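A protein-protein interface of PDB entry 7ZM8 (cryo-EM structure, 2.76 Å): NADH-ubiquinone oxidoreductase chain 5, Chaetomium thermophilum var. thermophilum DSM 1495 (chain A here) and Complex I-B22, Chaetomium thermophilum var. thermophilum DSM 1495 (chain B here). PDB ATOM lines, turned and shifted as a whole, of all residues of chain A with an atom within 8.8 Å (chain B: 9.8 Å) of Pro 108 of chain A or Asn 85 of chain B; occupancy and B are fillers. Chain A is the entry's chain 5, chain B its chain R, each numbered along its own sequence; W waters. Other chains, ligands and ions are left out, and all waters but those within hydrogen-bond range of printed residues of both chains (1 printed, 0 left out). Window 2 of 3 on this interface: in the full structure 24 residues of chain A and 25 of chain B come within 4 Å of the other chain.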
ATOM      1  N   GLY A  24      -3.021  36.101  31.599  1.00  0.00           N
ATOM      2  CA  GLY A  24      -1.829  36.119  30.740  1.00  0.00           C
ATOM      3  C   GLY A  24      -0.672  35.350  31.341  1.00  0.00           C
ATOM      4  O   GLY A  24      -0.852  34.756  32.406  1.00  0.00           O
ATOM      5  N   VAL A  25       0.464  35.327  30.648  1.00  0.00           N
ATOM      6  CA  VAL A  25       1.653  34.570  31.122  1.00  0.00           C
ATOM      7  C   VAL A  25       2.139  35.197  32.425  1.00  0.00           C
ATOM      8  O   VAL A  25       2.395  34.455  33.372  1.00  0.00           O
ATOM      9  CB  VAL A  25       2.748  34.608  30.043  1.00  0.00           C
ATOM     10  CG1 VAL A  25       4.026  33.927  30.500  1.00  0.00           C
ATOM     11  CG2 VAL A  25       2.270  34.049  28.715  1.00  0.00           C
ATOM     12  N   MET A 104      11.251  28.352  31.327  1.00  0.00           N
ATOM     13  CA  MET A 104      10.150  28.137  30.363  1.00  0.00           C
ATOM     14  C   MET A 104       9.697  29.474  29.779  1.00  0.00           C
ATOM     15  O   MET A 104       8.578  29.543  29.288  1.00  0.00           O
ATOM     16  CB  MET A 104       9.004  27.366  31.032  1.00  0.00           C
ATOM     17  CG  MET A 104       9.383  25.982  31.521  1.00  0.00           C
ATOM     18  SD  MET A 104       9.330  24.718  30.227  1.00  0.00           S
ATOM     19  CE  MET A 104       7.623  24.845  29.708  1.00  0.00           C
ATOM     20  N   SER A 105      10.566  30.479  29.794  1.00  0.00           N
ATOM     21  CA  SER A 105      10.235  31.831  29.273  1.00  0.00           C
ATOM     22  C   SER A 105       9.894  31.801  27.784  1.00  0.00           C
ATOM     23  O   SER A 105       8.912  32.458  27.400  1.00  0.00           O
ATOM     24  CB  SER A 105      11.374  32.754  29.532  1.00  0.00           C
ATOM     25  OG  SER A 105      12.585  32.191  29.058  1.00  0.00           O
ATOM     26  N   SER A 106      10.647  31.047  26.989  1.00  0.00           N
ATOM     27  CA  SER A 106      10.455  31.019  25.522  1.00  0.00           C
ATOM     28  C   SER A 106       9.331  30.078  25.095  1.00  0.00           C
ATOM     29  O   SER A 106       8.933  30.154  23.927  1.00  0.00           O
ATOM     30  CB  SER A 106      11.738  30.628  24.873  1.00  0.00           C
ATOM     31  OG  SER A 106      12.782  31.509  25.262  1.00  0.00           O
ATOM     32  N   ASP A 107       8.864  29.208  25.982  1.00  0.00           N
ATOM     33  CA  ASP A 107       7.849  28.202  25.588  1.00  0.00           C
ATOM     34  C   ASP A 107       6.557  28.921  25.264  1.00  0.00           C
ATOM     35  O   ASP A 107       6.242  29.863  25.971  1.00  0.00           O
ATOM     36  CB  ASP A 107       7.543  27.217  26.715  1.00  0.00           C
ATOM     37  CG  ASP A 107       6.858  25.952  26.233  1.00  0.00           C
ATOM     38  OD1 ASP A 107       7.559  25.101  25.672  1.00  0.00           O
ATOM     39  OD2 ASP A 107       5.628  25.848  26.386  1.00  0.00           O
ATOM     40  N   PRO A 108       5.770  28.491  24.266  1.00  0.00           N
ATOM     41  CA  PRO A 108       4.472  29.113  24.047  1.00  0.00           C
ATOM     42  C   PRO A 108       3.438  28.969  25.176  1.00  0.00           C
ATOM     43  O   PRO A 108       2.873  29.920  25.595  1.00  0.00           O
ATOM     44  CB  PRO A 108       3.973  28.390  22.787  1.00  0.00           C
ATOM     45  CG  PRO A 108       5.181  27.760  22.156  1.00  0.00           C
ATOM     46  CD  PRO A 108       6.114  27.455  23.301  1.00  0.00           C
ATOM     47  N   HIS A 109       3.349  27.821  25.812  1.00  0.00           N
ATOM     48  CA  HIS A 109       2.245  27.556  26.728  1.00  0.00           C
ATOM     49  C   HIS A 109       2.745  27.593  28.164  1.00  0.00           C
ATOM     50  O   HIS A 109       3.079  26.570  28.753  1.00  0.00           O
ATOM     51  CB  HIS A 109       1.610  26.221  26.373  1.00  0.00           C
ATOM     52  CG  HIS A 109       1.535  25.982  24.898  1.00  0.00           C
ATOM     53  ND1 HIS A 109       0.843  26.811  24.046  1.00  0.00           N
ATOM     54  CD2 HIS A 109       2.090  25.026  24.121  1.00  0.00           C
ATOM     55  CE1 HIS A 109       0.962  26.369  22.810  1.00  0.00           C
ATOM     56  NE2 HIS A 109       1.709  25.282  22.829  1.00  0.00           N
ATOM     57  N   ASN A 110       2.781  28.788  28.743  1.00  0.00           N
ATOM     58  CA  ASN A 110       3.219  28.943  30.123  1.00  0.00           C
ATOM     59  C   ASN A 110       2.084  28.795  31.116  1.00  0.00           C
ATOM     60  O   ASN A 110       2.292  28.267  32.209  1.00  0.00           O
ATOM     61  CB  ASN A 110       3.902  30.295  30.321  1.00  0.00           C
ATOM     62  CG  ASN A 110       5.235  30.370  29.638  1.00  0.00           C
ATOM     63  OD1 ASN A 110       5.567  31.379  29.035  1.00  0.00           O
ATOM     64  ND2 ASN A 110       6.014  29.307  29.731  1.00  0.00           N
ATOM     65  N   GLN A 111       0.890  29.271  30.768  1.00  0.00           N
ATOM     66  CA  GLN A 111      -0.238  29.143  31.679  1.00  0.00           C
ATOM     67  C   GLN A 111      -0.566  27.681  31.938  1.00  0.00           C
ATOM     68  O   GLN A 111      -0.821  27.289  33.080  1.00  0.00           O
ATOM     69  CB  GLN A 111      -1.454  29.882  31.124  1.00  0.00           C
ATOM     70  CG  GLN A 111      -1.292  31.386  31.046  1.00  0.00           C
ATOM     71  CD  GLN A 111      -0.865  31.850  29.679  1.00  0.00           C
ATOM     72  OE1 GLN A 111       0.201  31.486  29.195  1.00  0.00           O
ATOM     73  NE2 GLN A 111      -1.700  32.651  29.037  1.00  0.00           N
ATOM     74  N   ARG A 112      -0.544  26.854  30.894  1.00  0.00           N
ATOM     75  CA  ARG A 112      -0.820  25.434  31.077  1.00  0.00           C
ATOM     76  C   ARG A 112       0.261  24.756  31.904  1.00  0.00           C
ATOM     77  O   ARG A 112      -0.038  23.886  32.726  1.00  0.00           O
ATOM     78  CB  ARG A 112      -0.966  24.745  29.724  1.00  0.00           C
ATOM     79  CG  ARG A 112      -1.207  23.266  29.842  1.00  0.00           C
ATOM     80  CD  ARG A 112      -1.794  22.707  28.592  1.00  0.00           C
ATOM     81  NE  ARG A 112      -1.058  23.150  27.420  1.00  0.00           N
ATOM     82  CZ  ARG A 112      -0.047  22.490  26.870  1.00  0.00           C
ATOM     83  NH1 ARG A 112       0.549  22.982  25.800  1.00  0.00           N
ATOM     84  NH2 ARG A 112       0.369  21.344  27.387  1.00  0.00           N
ATOM     85  N   PHE A 113       1.523  25.135  31.698  1.00  0.00           N
ATOM     86  CA  PHE A 113       2.620  24.556  32.465  1.00  0.00           C
ATOM     87  C   PHE A 113       2.510  24.900  33.943  1.00  0.00           C
ATOM     88  O   PHE A 113       2.566  24.016  34.802  1.00  0.00           O
ATOM     89  CB  PHE A 113       3.952  25.044  31.904  1.00  0.00           C
ATOM     90  CG  PHE A 113       5.150  24.490  32.612  1.00  0.00           C
ATOM     91  CD1 PHE A 113       5.600  23.215  32.334  1.00  0.00           C
ATOM     92  CD2 PHE A 113       5.833  25.247  33.547  1.00  0.00           C
ATOM     93  CE1 PHE A 113       6.695  22.709  32.973  1.00  0.00           C
ATOM     94  CE2 PHE A 113       6.926  24.738  34.190  1.00  0.00           C
ATOM     95  CZ  PHE A 113       7.361  23.470  33.903  1.00  0.00           C
ATOM     96  N   PHE A 153       3.908  17.090  28.391  1.00  0.00           N
ATOM     97  CA  PHE A 153       3.620  18.533  28.199  1.00  0.00           C
ATOM     98  C   PHE A 153       3.818  18.902  26.725  1.00  0.00           C
ATOM     99  O   PHE A 153       2.980  19.605  26.153  1.00  0.00           O
ATOM    100  CB  PHE A 153       4.361  19.374  29.237  1.00  0.00           C
ATOM    101  CG  PHE A 153       4.215  20.855  29.010  1.00  0.00           C
ATOM    102  CD1 PHE A 153       3.048  21.515  29.363  1.00  0.00           C
ATOM    103  CD2 PHE A 153       5.231  21.581  28.415  1.00  0.00           C
ATOM    104  CE1 PHE A 153       2.905  22.871  29.128  1.00  0.00           C
ATOM    105  CE2 PHE A 153       5.086  22.936  28.187  1.00  0.00           C
ATOM    106  CZ  PHE A 153       3.927  23.576  28.544  1.00  0.00           C
ATOM    107  N   TRP A 154       4.893  18.397  26.118  1.00  0.00           N
ATOM    108  CA  TRP A 154       5.089  18.595  24.658  1.00  0.00           C
ATOM    109  C   TRP A 154       4.450  17.402  23.945  1.00  0.00           C
ATOM    110  O   TRP A 154       5.182  16.453  23.628  1.00  0.00           O
ATOM    111  CB  TRP A 154       6.576  18.751  24.330  1.00  0.00           C
ATOM    112  CG  TRP A 154       7.214  19.946  24.964  1.00  0.00           C
ATOM    113  CD1 TRP A 154       6.806  21.244  24.867  1.00  0.00           C
ATOM    114  CD2 TRP A 154       8.397  19.960  25.782  1.00  0.00           C
ATOM    115  NE1 TRP A 154       7.645  22.060  25.574  1.00  0.00           N
ATOM    116  CE2 TRP A 154       8.631  21.303  26.146  1.00  0.00           C
ATOM    117  CE3 TRP A 154       9.277  18.974  26.241  1.00  0.00           C
ATOM    118  CZ2 TRP A 154       9.707  21.679  26.946  1.00  0.00           C
ATOM    119  CZ3 TRP A 154      10.339  19.346  27.034  1.00  0.00           C
ATOM    120  CH2 TRP A 154      10.551  20.682  27.375  1.00  0.00           C
ATOM    121  N   PHE A 155       3.136  17.454  23.712  1.00  0.00           N
ATOM    122  CA  PHE A 155       2.381  16.314  23.120  1.00  0.00           C
ATOM    123  C   PHE A 155       2.797  16.020  21.673  1.00  0.00           C
ATOM    124  O   PHE A 155       2.550  14.903  21.200  1.00  0.00           O
ATOM    125  CB  PHE A 155       0.879  16.547  23.272  1.00  0.00           C
ATOM    126  CG  PHE A 155       0.437  17.980  23.127  1.00  0.00           C
ATOM    127  CD1 PHE A 155       0.334  18.568  21.876  1.00  0.00           C
ATOM    128  CD2 PHE A 155       0.113  18.736  24.241  1.00  0.00           C
ATOM    129  CE1 PHE A 155      -0.074  19.885  21.745  1.00  0.00           C
ATOM    130  CE2 PHE A 155      -0.297  20.052  24.107  1.00  0.00           C
ATOM    131  CZ  PHE A 155      -0.386  20.623  22.860  1.00  0.00           C
ATOM    132  N   THR A 156       3.365  17.005  20.981  1.00  0.00           N
ATOM    133  CA  THR A 156       3.787  16.826  19.568  1.00  0.00           C
ATOM    134  C   THR A 156       4.859  15.732  19.475  1.00  0.00           C
ATOM    135  O   THR A 156       4.874  15.024  18.463  1.00  0.00           O
ATOM    136  CB  THR A 156       4.130  18.169  18.914  1.00  0.00           C
ATOM    137  OG1 THR A 156       5.083  18.834  19.741  1.00  0.00           O
ATOM    138  CG2 THR A 156       2.916  19.053  18.740  1.00  0.00           C
ATOM    139  N   ARG A 157       5.745  15.628  20.470  1.00  0.00           N
ATOM    140  CA  ARG A 157       6.836  14.620  20.430  1.00  0.00           C
ATOM    141  C   ARG A 157       6.289  13.236  20.801  1.00  0.00           C
ATOM    142  O   ARG A 157       5.723  13.100  21.898  1.00  0.00           O
ATOM    143  CB  ARG A 157       7.976  15.082  21.340  1.00  0.00           C
ATOM    144  CG  ARG A 157       9.095  14.074  21.538  1.00  0.00           C
ATOM    145  CD  ARG A 157      10.210  14.774  22.287  1.00  0.00           C
ATOM    146  NE  ARG A 157      11.223  13.873  22.810  1.00  0.00           N
ATOM    147  CZ  ARG A 157      12.270  13.446  22.119  1.00  0.00           C
ATOM    148  NH1 ARG A 157      13.145  12.630  22.680  1.00  0.00           N
ATOM    149  NH2 ARG A 157      12.429  13.828  20.866  1.00  0.00           N
ATOM    150  N   PRO A 240       9.798  18.567  30.839  1.00  0.00           N
ATOM    151  CA  PRO A 240      10.783  19.613  30.968  1.00  0.00           C
ATOM    152  C   PRO A 240      11.598  19.454  32.256  1.00  0.00           C
ATOM    153  O   PRO A 240      11.142  18.792  33.154  1.00  0.00           O
ATOM    154  CB  PRO A 240       9.897  20.859  30.977  1.00  0.00           C
ATOM    155  CG  PRO A 240       8.608  20.441  30.319  1.00  0.00           C
ATOM    156  CD  PRO A 240       8.417  19.012  30.758  1.00  0.00           C
ATOM    157  N   ASP A 352      20.331  23.151  24.530  1.00  0.00           N
ATOM    158  CA  ASP A 352      19.461  21.970  24.739  1.00  0.00           C
ATOM    159  C   ASP A 352      20.170  20.686  24.347  1.00  0.00           C
ATOM    160  O   ASP A 352      19.498  19.765  23.939  1.00  0.00           O
ATOM    161  CB  ASP A 352      18.085  22.132  24.092  1.00  0.00           C
ATOM    162  CG  ASP A 352      17.030  22.709  25.020  1.00  0.00           C
ATOM    163  OD1 ASP A 352      17.286  22.771  26.236  1.00  0.00           O
ATOM    164  OD2 ASP A 352      15.960  23.093  24.516  1.00  0.00           O
ATOM    165  N   THR B  75      18.276  18.315  17.801  1.00  0.00           N
ATOM    166  CA  THR B  75      17.104  18.648  16.963  1.00  0.00           C
ATOM    167  C   THR B  75      16.918  17.620  15.850  1.00  0.00           C
ATOM    168  O   THR B  75      15.959  17.751  15.084  1.00  0.00           O
ATOM    169  CB  THR B  75      17.325  20.056  16.408  1.00  0.00           C
ATOM    170  OG1 THR B  75      16.296  20.365  15.469  1.00  0.00           O
ATOM    171  CG2 THR B  75      18.689  20.211  15.772  1.00  0.00           C
ATOM    172  N   SER B  80      16.740  14.926  21.450  1.00  0.00           N
ATOM    173  CA  SER B  80      15.954  15.367  22.627  1.00  0.00           C
ATOM    174  C   SER B  80      14.887  16.432  22.340  1.00  0.00           C
ATOM    175  O   SER B  80      13.861  16.398  23.019  1.00  0.00           O
ATOM    176  CB  SER B  80      16.910  15.763  23.705  1.00  0.00           C
ATOM    177  OG  SER B  80      17.658  14.642  24.141  1.00  0.00           O
ATOM    178  N   LYS B  81      15.139  17.358  21.415  1.00  0.00           N
ATOM    179  CA  LYS B  81      14.200  18.486  21.194  1.00  0.00           C
ATOM    180  C   LYS B  81      13.468  18.245  19.878  1.00  0.00           C
ATOM    181  O   LYS B  81      12.748  19.133  19.413  1.00  0.00           O
ATOM    182  CB  LYS B  81      15.029  19.772  21.145  1.00  0.00           C
ATOM    183  CG  LYS B  81      14.268  21.065  21.392  1.00  0.00           C
ATOM    184  CD  LYS B  81      15.106  22.295  21.170  1.00  0.00           C
ATOM    185  CE  LYS B  81      14.300  23.575  21.230  1.00  0.00           C
ATOM    186  NZ  LYS B  81      13.716  23.793  22.574  1.00  0.00           N
ATOM    187  N   TYR B  82      13.626  17.047  19.330  1.00  0.00           N
ATOM    188  CA  TYR B  82      12.965  16.703  18.053  1.00  0.00           C
ATOM    189  C   TYR B  82      11.447  16.718  18.243  1.00  0.00           C
ATOM    190  O   TYR B  82      10.979  16.065  19.183  1.00  0.00           O
ATOM    191  CB  TYR B  82      13.451  15.333  17.590  1.00  0.00           C
ATOM    192  CG  TYR B  82      12.941  14.927  16.234  1.00  0.00           C
ATOM    193  CD1 TYR B  82      13.143  15.732  15.128  1.00  0.00           C
ATOM    194  CD2 TYR B  82      12.248  13.744  16.061  1.00  0.00           C
ATOM    195  CE1 TYR B  82      12.676  15.369  13.877  1.00  0.00           C
ATOM    196  CE2 TYR B  82      11.776  13.366  14.818  1.00  0.00           C
ATOM    197  CZ  TYR B  82      11.991  14.178  13.723  1.00  0.00           C
ATOM    198  OH  TYR B  82      11.525  13.804  12.498  1.00  0.00           O
ATOM    199  N   GLU B  83      10.726  17.406  17.355  1.00  0.00           N
ATOM    200  CA  GLU B  83       9.244  17.463  17.401  1.00  0.00           C
ATOM    201  C   GLU B  83       8.727  18.114  18.686  1.00  0.00           C
ATOM    202  O   GLU B  83       7.607  17.786  19.061  1.00  0.00           O
ATOM    203  CB  GLU B  83       8.685  16.057  17.199  1.00  0.00           C
ATOM    204  CG  GLU B  83       8.985  15.499  15.826  1.00  0.00           C
ATOM    205  CD  GLU B  83       8.464  14.097  15.589  1.00  0.00           C
ATOM    206  OE1 GLU B  83       8.048  13.451  16.568  1.00  0.00           O
ATOM    207  OE2 GLU B  83       8.470  13.659  14.425  1.00  0.00           O
ATOM    208  N   ARG B  84       9.470  19.042  19.301  1.00  0.00           N
ATOM    209  CA  ARG B  84       9.051  19.580  20.618  1.00  0.00           C
ATOM    210  C   ARG B  84       7.891  20.565  20.513  1.00  0.00           C
ATOM    211  O   ARG B  84       6.872  20.357  21.222  1.00  0.00           O
ATOM    212  CB  ARG B  84      10.214  20.179  21.406  1.00  0.00           C
ATOM    213  CG  ARG B  84       9.792  21.109  22.530  1.00  0.00           C
ATOM    214  CD  ARG B  84      10.965  21.470  23.409  1.00  0.00           C
ATOM    215  NE  ARG B  84      11.662  20.266  23.833  1.00  0.00           N
ATOM    216  CZ  ARG B  84      12.755  20.260  24.577  1.00  0.00           C
ATOM    217  NH1 ARG B  84      13.276  21.398  24.994  1.00  0.00           N
ATOM    218  NH2 ARG B  84      13.324  19.119  24.902  1.00  0.00           N
ATOM    219  N   ASN B  85       7.960  21.538  19.629  1.00  0.00           N
ATOM    220  CA  ASN B  85       6.805  22.448  19.577  1.00  0.00           C
ATOM    221  C   ASN B  85       6.459  22.486  18.105  1.00  0.00           C
ATOM    222  O   ASN B  85       6.554  23.562  17.502  1.00  0.00           O
ATOM    223  CB  ASN B  85       7.170  23.797  20.205  1.00  0.00           C
ATOM    224  CG  ASN B  85       6.983  23.861  21.705  1.00  0.00           C
ATOM    225  OD1 ASN B  85       5.894  23.620  22.215  1.00  0.00           O
ATOM    226  ND2 ASN B  85       8.033  24.222  22.418  1.00  0.00           N
ATOM    227  N   LEU B  86       6.082  21.330  17.559  1.00  0.00           N
ATOM    228  CA  LEU B  86       5.844  21.249  16.106  1.00  0.00           C
ATOM    229  C   LEU B  86       4.651  22.129  15.779  1.00  0.00           C
ATOM    230  O   LEU B  86       3.596  21.930  16.405  1.00  0.00           O
ATOM    231  CB  LEU B  86       5.601  19.798  15.706  1.00  0.00           C
ATOM    232  CG  LEU B  86       6.825  19.008  15.267  1.00  0.00           C
ATOM    233  CD1 LEU B  86       6.398  17.719  14.592  1.00  0.00           C
ATOM    234  CD2 LEU B  86       7.693  19.833  14.335  1.00  0.00           C
ATOM    235  N   PRO B  87       4.776  23.065  14.814  1.00  0.00           N
ATOM    236  CA  PRO B  87       3.694  23.993  14.496  1.00  0.00           C
ATOM    237  C   PRO B  87       2.483  23.294  13.875  1.00  0.00           C
ATOM    238  O   PRO B  87       2.684  22.270  13.280  1.00  0.00           O
ATOM    239  CB  PRO B  87       4.386  25.000  13.569  1.00  0.00           C
ATOM    240  CG  PRO B  87       5.478  24.202  12.908  1.00  0.00           C
ATOM    241  CD  PRO B  87       5.972  23.285  14.002  1.00  0.00           C
ATOM    242  N   VAL B  88       1.273  23.840  14.032  1.00  0.00           N
ATOM    243  CA  VAL B  88       0.136  23.265  13.307  1.00  0.00           C
ATOM    244  C   VAL B  88       0.439  23.290  11.814  1.00  0.00           C
ATOM    245  O   VAL B  88       0.883  24.329  11.290  1.00  0.00           O
ATOM    246  CB  VAL B  88      -1.152  24.045  13.624  1.00  0.00           C
ATOM    247  CG1 VAL B  88      -2.316  23.504  12.836  1.00  0.00           C
ATOM    248  CG2 VAL B  88      -1.449  23.993  15.112  1.00  0.00           C
ATOM    249  N   PRO B  89       0.249  22.190  11.087  1.00  0.00           N
ATOM    250  CA  PRO B  89       0.531  22.185   9.648  1.00  0.00           C
ATOM    251  C   PRO B  89      -0.533  22.855   8.795  1.00  0.00           C
ATOM    252  O   PRO B  89      -0.512  22.689   7.574  1.00  0.00           O
ATOM    253  CB  PRO B  89       0.611  20.682   9.321  1.00  0.00           C
ATOM    254  CG  PRO B  89       0.525  19.957  10.635  1.00  0.00           C
ATOM    255  CD  PRO B  89      -0.162  20.867  11.572  1.00  0.00           C
HETATM  256  O   HOH W   1       5.315  13.599  16.359  1.00  0.00           O
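Water W1 bridges the backbone carbonyl oxygen (O) of Thr 156 of chain A (2.6 Å) and the side-chain carboxylate (OE1) of Glu 83 of chain B (2.7 Å).
The side-chain amino group (NZ) of Lys 81 of chain B is in salt-bridge range of the side-chain carboxylate (OD2) of Asp 352 of chain A (3.0 Å).
The guanidinium group of Arg 157 of chain A is in hydrogen-bond range of the backbone carbonyl oxygen of Tyr 82 of chain B, 3.2 Å away.
O of Glu 83 of chain B sits at hydrogen-bond distance from OG1 of Thr 156 of chain A (2.8 Å).
The backbone NH (N) of Arg 157 of chain A sits at hydrogen-bond distance from the backbone carbonyl oxygen (O) of Glu 83 of chain B (3.2 Å).
OG1 of Thr 156 of chain A is in hydrogen-bond range of O of Arg 84 of chain B (2.8 Å).
OD2 of Asp 352 of chain A is in salt-bridge range of NH1 of Arg 84 of chain B.
The side-chain amide nitrogen (ND2) of Asn 85 of chain B lies within hydrogen-bond range of the side-chain carboxylate (OD1) of Asp 107 of chain A.
The backbone NH (N) of Leu 86 of chain B lies within hydrogen-bond range of the side-chain hydroxyl (OG1) of Thr 156 of chain A, 3.5 Å away.
Hydrophobic or aromatic side chains of chain A that line the printed part of chain B: Pro 108 and Trp 154.
Among the printed residues, 13 pairs touch across the chains.
Among the printed residues, Asp or Glu carboxylates within 4 Å of a Lys or Arg side-chain nitrogen of the other chain: Asp 352 of chain A with Lys 81 of chain B and Asp 352 of chain A with Arg 84 of chain B.
Printed residues of chain B within 4 Å of Asp 107 of chain A: Asn 85.
Of chain B, only Asn 85 comes within 4 Å of Pro 108 of chain A.
No residue of chain B comes within 4 Å of His 109 of chain A.
Of the printed residues of chain B, Thr 156 of chain A touches Glu 83, Arg 84, Asn 85 and Leu 86.
Of the printed residues of chain A, Tyr 82 of chain B touches Arg 157.
Printed residues of chain A within 4 Å of Glu 83 of chain B: Thr 156 and Arg 157.
Of chain A, only Asp 107 (3.4 Å), Pro 108 (3.9 Å), Trp 154 (3.7 Å) and Thr 156 (3.9 Å) come within 4 Å of Asn 85 of chain B.
The nearest residue of chain B that does not touch Pro 108 of chain A is Arg 84 of chain B (7.4 Å).
Among the printed residues, merely in contact across the chains: Arg 157 of chain A with Ser 80 of chain B, Trp 154 of chain A with Arg 84 of chain B, Trp 154 of chain A with Asn 85 of chain B, Pro 108 of chain A with Asn 85 of chain B and Thr 156 of chain A with Asn 85 of chain B.
The backbone carbonyl oxygen (O) of Ser 80 of chain B is in hydrogen-bond range of the guanidinium group (NH2) of Arg 84 of chain B (3.4 Å).
The backbone NH (N) of His 109 of chain A lies within hydrogen-bond range of the side-chain carboxylate (OD2) of Asp 107 of chain A.
O of Asp 107 of chain A lies close to OD1 of Asn 110 of chain A (3.5 Å).
The side-chain carboxylate (OD1) of Asp 107 of chain A sits at hydrogen-bond distance from the indole nitrogen (NE1) of Trp 154 of chain A.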
